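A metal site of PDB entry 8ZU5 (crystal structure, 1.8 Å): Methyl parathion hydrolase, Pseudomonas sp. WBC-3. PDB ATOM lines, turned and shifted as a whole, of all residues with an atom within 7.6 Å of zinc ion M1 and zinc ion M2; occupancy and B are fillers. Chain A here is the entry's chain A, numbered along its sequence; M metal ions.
ND1 of His 199 lies within hydrogen-bond range of OD1 of Asp 239, 2.8 Å away. The side-chain hydroxyl (OG) of Ser 266 sits close to the side-chain carboxylate (OD1) of Asp 220 (3.5 Å). A ring nitrogen (NE2) of His 203 sits at hydrogen-bond distance from the backbone NH of Asp 220 (2.9 Å). A ring nitrogen (ND1) of His 267 sits at hydrogen-bond distance from the backbone carbonyl oxygen (O) of Ser 61 (2.8 Å). The side-chain carboxylate (OD2) of Asp 77 is in hydrogen-bond range of a ring nitrogen (ND1) of His 117. ND1 of His 112 sits at hydrogen-bond distance from OG1 of Thr 111 (3.0 Å).
The nearest printed residue that does not touch zinc ion M1 is His 117 (4.2 Å).
Four residues have an atom within 4 Å of zinc ion M2: Asp 116, His 117, Asp 220 and His 267.
A ring nitrogen (NE2) of His 199 is bound to zinc ion M1 (2.2 Å). Zinc ion M1 is bound by OD2 of Asp 220 (2.2 Å). ND1 of His 114 binds zinc ion M1 (2.3 Å). Zinc ion M1 is bound by NE2 of His 112. Zinc ion M1 has four donor atoms within binding distance.
OD2 of Asp 116 binds zinc ion M2, at 2.2 Å. Zinc ion M2 is bound by NE2 of His 267. Zinc ion M2 is bound by OD2 of Asp 220 (2.3 Å). NE2 of His 117 binds zinc ion M2 (2.3 Å).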
ATOM      1  N   LEU A  32      11.354 -14.853  12.121  1.00  0.00           N
ATOM      2  CA  LEU A  32      10.839 -14.372  13.405  1.00  0.00           C
ATOM      3  C   LEU A  32       9.319 -14.477  13.468  1.00  0.00           C
ATOM      4  O   LEU A  32       8.635 -14.126  12.491  1.00  0.00           O
ATOM      5  CB  LEU A  32      11.263 -12.919  13.690  1.00  0.00           C
ATOM      6  CG  LEU A  32      12.768 -12.628  13.754  1.00  0.00           C
ATOM      7  CD1 LEU A  32      13.097 -11.152  14.018  1.00  0.00           C
ATOM      8  CD2 LEU A  32      13.415 -13.525  14.810  1.00  0.00           C
ATOM      9  N   THR A  60      13.690 -12.174   8.490  1.00  0.00           N
ATOM     10  CA  THR A  60      14.049 -10.809   8.902  1.00  0.00           C
ATOM     11  C   THR A  60      15.556 -10.617   8.727  1.00  0.00           C
ATOM     12  O   THR A  60      16.349 -11.386   9.287  1.00  0.00           O
ATOM     13  CB  THR A  60      13.635 -10.549  10.344  1.00  0.00           C
ATOM     14  OG1 THR A  60      12.240 -10.838  10.531  1.00  0.00           O
ATOM     15  CG2 THR A  60      13.948  -9.092  10.749  1.00  0.00           C
ATOM     16  N   SER A  61      15.963  -9.612   7.946  1.00  0.00           N
ATOM     17  CA  SER A  61      17.413  -9.484   7.877  1.00  0.00           C
ATOM     18  C   SER A  61      17.991  -8.776   9.113  1.00  0.00           C
ATOM     19  O   SER A  61      17.274  -8.180   9.912  1.00  0.00           O
ATOM     20  CB  SER A  61      17.871  -8.880   6.531  1.00  0.00           C
ATOM     21  OG  SER A  61      17.009  -7.957   5.916  1.00  0.00           O
ATOM     22  N   VAL A  62      19.299  -8.955   9.298  1.00  0.00           N
ATOM     23  CA  VAL A  62      20.068  -8.412  10.429  1.00  0.00           C
ATOM     24  C   VAL A  62      21.272  -7.742   9.805  1.00  0.00           C
ATOM     25  O   VAL A  62      22.078  -8.426   9.164  1.00  0.00           O
ATOM     26  CB  VAL A  62      20.531  -9.519  11.403  1.00  0.00           C
ATOM     27  CG1 VAL A  62      21.451  -8.931  12.545  1.00  0.00           C
ATOM     28  CG2 VAL A  62      19.310 -10.340  11.942  1.00  0.00           C
ATOM     29  N   ASP A  77      26.910  -1.477  14.957  1.00  0.00           N
ATOM     30  CA  ASP A  77      26.349  -2.798  15.225  1.00  0.00           C
ATOM     31  C   ASP A  77      27.088  -3.893  14.461  1.00  0.00           C
ATOM     32  O   ASP A  77      27.701  -3.623  13.422  1.00  0.00           O
ATOM     33  CB  ASP A  77      24.865  -2.819  14.918  1.00  0.00           C
ATOM     34  CG  ASP A  77      24.060  -1.943  15.857  1.00  0.00           C
ATOM     35  OD1 ASP A  77      24.608  -1.425  16.876  1.00  0.00           O
ATOM     36  OD2 ASP A  77      22.870  -1.744  15.533  1.00  0.00           O
ATOM     37  N   THR A 111      23.982   0.520  18.601  1.00  0.00           N
ATOM     38  CA  THR A 111      22.668   1.100  18.821  1.00  0.00           C
ATOM     39  C   THR A 111      22.094   0.597  20.134  1.00  0.00           C
ATOM     40  O   THR A 111      21.511   1.373  20.907  1.00  0.00           O
ATOM     41  CB  THR A 111      21.714   0.833  17.651  1.00  0.00           C
ATOM     42  OG1 THR A 111      21.521  -0.557  17.493  1.00  0.00           O
ATOM     43  CG2 THR A 111      22.299   1.467  16.339  1.00  0.00           C
ATOM     44  N   HIS A 112      22.329  -0.667  20.460  1.00  0.00           N
ATOM     45  CA  HIS A 112      21.890  -1.282  21.707  1.00  0.00           C
ATOM     46  C   HIS A 112      22.546  -2.642  21.811  1.00  0.00           C
ATOM     47  O   HIS A 112      23.239  -3.077  20.885  1.00  0.00           O
ATOM     48  CB  HIS A 112      20.374  -1.386  21.783  1.00  0.00           C
ATOM     49  CG  HIS A 112      19.757  -2.327  20.776  1.00  0.00           C
ATOM     50  ND1 HIS A 112      19.895  -2.162  19.425  1.00  0.00           N
ATOM     51  CD2 HIS A 112      18.881  -3.352  20.943  1.00  0.00           C
ATOM     52  CE1 HIS A 112      19.158  -3.066  18.795  1.00  0.00           C
ATOM     53  NE2 HIS A 112      18.536  -3.808  19.703  1.00  0.00           N
ATOM     54  N   MET A 113      22.265  -3.355  22.908  1.00  0.00           N
ATOM     55  CA  MET A 113      23.079  -4.510  23.265  1.00  0.00           C
ATOM     56  C   MET A 113      22.360  -5.851  23.099  1.00  0.00           C
ATOM     57  O   MET A 113      22.789  -6.851  23.697  1.00  0.00           O
ATOM     58  CB  MET A 113      23.556  -4.314  24.690  1.00  0.00           C
ATOM     59  CG  MET A 113      24.663  -3.305  24.682  1.00  0.00           C
ATOM     60  SD  MET A 113      25.515  -3.070  26.212  1.00  0.00           S
ATOM     61  CE  MET A 113      26.531  -1.650  25.787  1.00  0.00           C
ATOM     62  N   HIS A 114      21.254  -5.894  22.348  1.00  0.00           N
ATOM     63  CA  HIS A 114      20.623  -7.190  22.054  1.00  0.00           C
ATOM     64  C   HIS A 114      21.605  -8.078  21.281  1.00  0.00           C
ATOM     65  O   HIS A 114      22.544  -7.567  20.658  1.00  0.00           O
ATOM     66  CB  HIS A 114      19.349  -6.980  21.240  1.00  0.00           C
ATOM     67  CG  HIS A 114      18.116  -6.678  22.054  1.00  0.00           C
ATOM     68  ND1 HIS A 114      16.950  -6.226  21.487  1.00  0.00           N
ATOM     69  CD2 HIS A 114      17.894  -6.735  23.392  1.00  0.00           C
ATOM     70  CE1 HIS A 114      16.057  -6.006  22.433  1.00  0.00           C
ATOM     71  NE2 HIS A 114      16.588  -6.331  23.597  1.00  0.00           N
ATOM     72  N   PRO A 115      21.427  -9.406  21.318  1.00  0.00           N
ATOM     73  CA  PRO A 115      22.484 -10.309  20.830  1.00  0.00           C
ATOM     74  C   PRO A 115      22.820 -10.180  19.362  1.00  0.00           C
ATOM     75  O   PRO A 115      23.973 -10.409  18.975  1.00  0.00           O
ATOM     76  CB  PRO A 115      21.923 -11.709  21.132  1.00  0.00           C
ATOM     77  CG  PRO A 115      20.896 -11.529  22.142  1.00  0.00           C
ATOM     78  CD  PRO A 115      20.291 -10.164  21.883  1.00  0.00           C
ATOM     79  N   ASP A 116      21.837  -9.844  18.530  1.00  0.00           N
ATOM     80  CA  ASP A 116      21.971  -9.694  17.086  1.00  0.00           C
ATOM     81  C   ASP A 116      22.614  -8.380  16.670  1.00  0.00           C
ATOM     82  O   ASP A 116      22.679  -8.061  15.465  1.00  0.00           O
ATOM     83  CB  ASP A 116      20.587  -9.866  16.423  1.00  0.00           C
ATOM     84  CG  ASP A 116      19.502  -9.018  17.075  1.00  0.00           C
ATOM     85  OD1 ASP A 116      19.287  -9.172  18.305  1.00  0.00           O
ATOM     86  OD2 ASP A 116      18.858  -8.189  16.368  1.00  0.00           O
ATOM     87  N   HIS A 117      23.095  -7.623  17.651  1.00  0.00           N
ATOM     88  CA  HIS A 117      23.834  -6.389  17.456  1.00  0.00           C
ATOM     89  C   HIS A 117      25.196  -6.402  18.144  1.00  0.00           C
ATOM     90  O   HIS A 117      26.116  -5.720  17.672  1.00  0.00           O
ATOM     91  CB  HIS A 117      23.012  -5.211  18.003  1.00  0.00           C
ATOM     92  CG  HIS A 117      21.712  -5.026  17.289  1.00  0.00           C
ATOM     93  ND1 HIS A 117      21.524  -4.039  16.343  1.00  0.00           N
ATOM     94  CD2 HIS A 117      20.537  -5.710  17.373  1.00  0.00           C
ATOM     95  CE1 HIS A 117      20.284  -4.107  15.892  1.00  0.00           C
ATOM     96  NE2 HIS A 117      19.677  -5.135  16.481  1.00  0.00           N
ATOM     97  N   TRP A 144      22.524  -3.708  30.747  1.00  0.00           N
ATOM     98  CA  TRP A 144      22.774  -5.063  30.260  1.00  0.00           C
ATOM     99  C   TRP A 144      23.974  -5.729  30.921  1.00  0.00           C
ATOM    100  O   TRP A 144      24.034  -6.965  30.937  1.00  0.00           O
ATOM    101  CB  TRP A 144      22.949  -5.066  28.737  1.00  0.00           C
ATOM    102  CG  TRP A 144      21.673  -4.719  28.008  1.00  0.00           C
ATOM    103  CD1 TRP A 144      21.424  -3.573  27.309  1.00  0.00           C
ATOM    104  CD2 TRP A 144      20.482  -5.531  27.892  1.00  0.00           C
ATOM    105  NE1 TRP A 144      20.128  -3.611  26.788  1.00  0.00           N
ATOM    106  CE2 TRP A 144      19.547  -4.799  27.125  1.00  0.00           C
ATOM    107  CE3 TRP A 144      20.119  -6.792  28.363  1.00  0.00           C
ATOM    108  CZ2 TRP A 144      18.274  -5.295  26.818  1.00  0.00           C
ATOM    109  CZ3 TRP A 144      18.856  -7.293  28.054  1.00  0.00           C
ATOM    110  CH2 TRP A 144      17.944  -6.539  27.292  1.00  0.00           C
ATOM    111  N   PHE A 161      19.913 -12.749  26.931  1.00  0.00           N
ATOM    112  CA  PHE A 161      20.285 -11.413  26.484  1.00  0.00           C
ATOM    113  C   PHE A 161      21.401 -10.846  27.351  1.00  0.00           C
ATOM    114  O   PHE A 161      22.400 -10.284  26.837  1.00  0.00           O
ATOM    115  CB  PHE A 161      19.086 -10.471  26.517  1.00  0.00           C
ATOM    116  CG  PHE A 161      18.048 -10.776  25.479  1.00  0.00           C
ATOM    117  CD1 PHE A 161      18.382 -11.436  24.322  1.00  0.00           C
ATOM    118  CD2 PHE A 161      16.728 -10.394  25.669  1.00  0.00           C
ATOM    119  CE1 PHE A 161      17.419 -11.716  23.357  1.00  0.00           C
ATOM    120  CE2 PHE A 161      15.768 -10.671  24.717  1.00  0.00           C
ATOM    121  CZ  PHE A 161      16.111 -11.336  23.559  1.00  0.00           C
ATOM    122  N   HIS A 199      13.390   1.150  23.138  1.00  0.00           N
ATOM    123  CA  HIS A 199      13.479  -0.283  22.736  1.00  0.00           C
ATOM    124  C   HIS A 199      14.358  -0.915  23.809  1.00  0.00           C
ATOM    125  O   HIS A 199      14.059  -2.039  24.243  1.00  0.00           O
ATOM    126  CB  HIS A 199      14.143  -0.399  21.366  1.00  0.00           C
ATOM    127  CG  HIS A 199      14.466  -1.794  20.946  1.00  0.00           C
ATOM    128  ND1 HIS A 199      13.502  -2.775  20.798  1.00  0.00           N
ATOM    129  CD2 HIS A 199      15.631  -2.357  20.624  1.00  0.00           C
ATOM    130  CE1 HIS A 199      14.089  -3.892  20.405  1.00  0.00           C
ATOM    131  NE2 HIS A 199      15.375  -3.667  20.295  1.00  0.00           N
ATOM    132  N   THR A 200      15.454  -0.232  24.177  1.00  0.00           N
ATOM    133  CA  THR A 200      16.295  -0.629  25.308  1.00  0.00           C
ATOM    134  C   THR A 200      16.522   0.637  26.105  1.00  0.00           C
ATOM    135  O   THR A 200      16.345   1.727  25.557  1.00  0.00           O
ATOM    136  CB  THR A 200      17.624  -1.236  24.836  1.00  0.00           C
ATOM    137  OG1 THR A 200      18.272  -0.248  24.050  1.00  0.00           O
ATOM    138  CG2 THR A 200      17.422  -2.526  24.052  1.00  0.00           C
ATOM    139  N   HIS A 203      19.017   2.706  23.997  1.00  0.00           N
ATOM    140  CA  HIS A 203      19.048   2.596  22.544  1.00  0.00           C
ATOM    141  C   HIS A 203      19.401   3.942  21.923  1.00  0.00           C
ATOM    142  O   HIS A 203      18.806   4.976  22.263  1.00  0.00           O
ATOM    143  CB  HIS A 203      17.701   2.141  21.992  1.00  0.00           C
ATOM    144  CG  HIS A 203      17.713   1.942  20.505  1.00  0.00           C
ATOM    145  ND1 HIS A 203      17.590   2.986  19.615  1.00  0.00           N
ATOM    146  CD2 HIS A 203      17.692   0.805  19.766  1.00  0.00           C
ATOM    147  CE1 HIS A 203      17.603   2.510  18.381  1.00  0.00           C
ATOM    148  NE2 HIS A 203      17.654   1.195  18.440  1.00  0.00           N
ATOM    149  N   GLY A 219      18.945   1.819  14.146  1.00  0.00           N
ATOM    150  CA  GLY A 219      18.993   0.646  14.993  1.00  0.00           C
ATOM    151  C   GLY A 219      17.674  -0.114  14.906  1.00  0.00           C
ATOM    152  O   GLY A 219      17.228  -0.493  13.810  1.00  0.00           O
ATOM    153  N   ASP A 220      17.048  -0.346  16.062  1.00  0.00           N
ATOM    154  CA  ASP A 220      15.800  -1.095  16.169  1.00  0.00           C
ATOM    155  C   ASP A 220      14.613  -0.200  16.494  1.00  0.00           C
ATOM    156  O   ASP A 220      13.702  -0.601  17.250  1.00  0.00           O
ATOM    157  CB  ASP A 220      15.957  -2.201  17.214  1.00  0.00           C
ATOM    158  CG  ASP A 220      16.687  -3.396  16.659  1.00  0.00           C
ATOM    159  OD1 ASP A 220      17.220  -3.276  15.552  1.00  0.00           O
ATOM    160  OD2 ASP A 220      16.761  -4.432  17.346  1.00  0.00           O
ATOM    161  N   LEU A 221      14.615   1.038  16.001  1.00  0.00           N
ATOM    162  CA  LEU A 221      13.418   1.859  16.184  1.00  0.00           C
ATOM    163  C   LEU A 221      12.249   1.340  15.376  1.00  0.00           C
ATOM    164  O   LEU A 221      11.119   1.751  15.642  1.00  0.00           O
ATOM    165  CB  LEU A 221      13.651   3.313  15.818  1.00  0.00           C
ATOM    166  CG  LEU A 221      14.385   4.191  16.823  1.00  0.00           C
ATOM    167  CD1 LEU A 221      14.510   5.603  16.264  1.00  0.00           C
ATOM    168  CD2 LEU A 221      13.523   4.174  18.074  1.00  0.00           C
ATOM    169  N   ILE A 222      12.498   0.498  14.380  1.00  0.00           N
ATOM    170  CA  ILE A 222      11.456  -0.236  13.678  1.00  0.00           C
ATOM    171  C   ILE A 222      11.911  -1.678  13.516  1.00  0.00           C
ATOM    172  O   ILE A 222      13.081  -1.955  13.220  1.00  0.00           O
ATOM    173  CB  ILE A 222      11.122   0.393  12.313  1.00  0.00           C
ATOM    174  CG1 ILE A 222       9.922  -0.331  11.705  1.00  0.00           C
ATOM    175  CG2 ILE A 222      12.317   0.350  11.384  1.00  0.00           C
ATOM    176  CD1 ILE A 222       9.316   0.381  10.538  1.00  0.00           C
ATOM    177  N   LEU A 223      10.998  -2.603  13.753  1.00  0.00           N
ATOM    178  CA  LEU A 223      11.294  -4.027  13.715  1.00  0.00           C
ATOM    179  C   LEU A 223      10.533  -4.765  12.616  1.00  0.00           C
ATOM    180  O   LEU A 223      11.080  -5.712  12.040  1.00  0.00           O
ATOM    181  CB  LEU A 223      10.967  -4.646  15.079  1.00  0.00           C
ATOM    182  CG  LEU A 223      11.819  -4.063  16.233  1.00  0.00           C
ATOM    183  CD1 LEU A 223      11.267  -4.467  17.623  1.00  0.00           C
ATOM    184  CD2 LEU A 223      13.324  -4.443  16.102  1.00  0.00           C
ATOM    185  N   LEU A 238       9.424  -7.047  22.999  1.00  0.00           N
ATOM    186  CA  LEU A 238      10.867  -6.837  23.135  1.00  0.00           C
ATOM    187  C   LEU A 238      11.226  -5.411  23.502  1.00  0.00           C
ATOM    188  O   LEU A 238      12.409  -5.158  23.824  1.00  0.00           O
ATOM    189  CB  LEU A 238      11.596  -7.147  21.841  1.00  0.00           C
ATOM    190  CG  LEU A 238      11.542  -8.506  21.173  1.00  0.00           C
ATOM    191  CD1 LEU A 238      12.253  -8.318  19.821  1.00  0.00           C
ATOM    192  CD2 LEU A 238      12.204  -9.550  22.068  1.00  0.00           C
ATOM    193  N   ASP A 239      10.290  -4.469  23.424  1.00  0.00           N
ATOM    194  CA  ASP A 239      10.594  -3.081  23.737  1.00  0.00           C
ATOM    195  C   ASP A 239      10.543  -2.852  25.238  1.00  0.00           C
ATOM    196  O   ASP A 239       9.541  -3.184  25.884  1.00  0.00           O
ATOM    197  CB  ASP A 239       9.653  -2.129  23.000  1.00  0.00           C
ATOM    198  CG  ASP A 239       9.748  -2.256  21.509  1.00  0.00           C
ATOM    199  OD1 ASP A 239      10.842  -1.967  20.977  1.00  0.00           O
ATOM    200  OD2 ASP A 239       8.719  -2.588  20.858  1.00  0.00           O
ATOM    201  N   SER A 266      18.282  -1.824  11.227  1.00  0.00           N
ATOM    202  CA  SER A 266      18.931  -3.135  11.288  1.00  0.00           C
ATOM    203  C   SER A 266      18.092  -4.233  10.655  1.00  0.00           C
ATOM    204  O   SER A 266      18.623  -5.174  10.046  1.00  0.00           O
ATOM    205  CB  SER A 266      19.209  -3.512  12.746  1.00  0.00           C
ATOM    206  OG  SER A 266      19.849  -2.458  13.470  1.00  0.00           O
ATOM    207  N   HIS A 267      16.769  -4.159  10.830  1.00  0.00           N
ATOM    208  CA  HIS A 267      15.880  -5.225  10.376  1.00  0.00           C
ATOM    209  C   HIS A 267      14.939  -4.826   9.257  1.00  0.00           C
ATOM    210  O   HIS A 267      14.008  -5.593   8.951  1.00  0.00           O
ATOM    211  CB  HIS A 267      15.099  -5.774  11.576  1.00  0.00           C
ATOM    212  CG  HIS A 267      15.999  -6.181  12.685  1.00  0.00           C
ATOM    213  ND1 HIS A 267      16.975  -7.150  12.526  1.00  0.00           N
ATOM    214  CD2 HIS A 267      16.137  -5.712  13.944  1.00  0.00           C
ATOM    215  CE1 HIS A 267      17.641  -7.290  13.656  1.00  0.00           C
ATOM    216  NE2 HIS A 267      17.164  -6.411  14.518  1.00  0.00           N
HETATM  217 ZN    ZN M   1      16.684  -5.219  19.442  1.00  0.00          ZN
HETATM  218 ZN    ZN M   2      17.764  -6.366  16.692  1.00  0.00          ZN
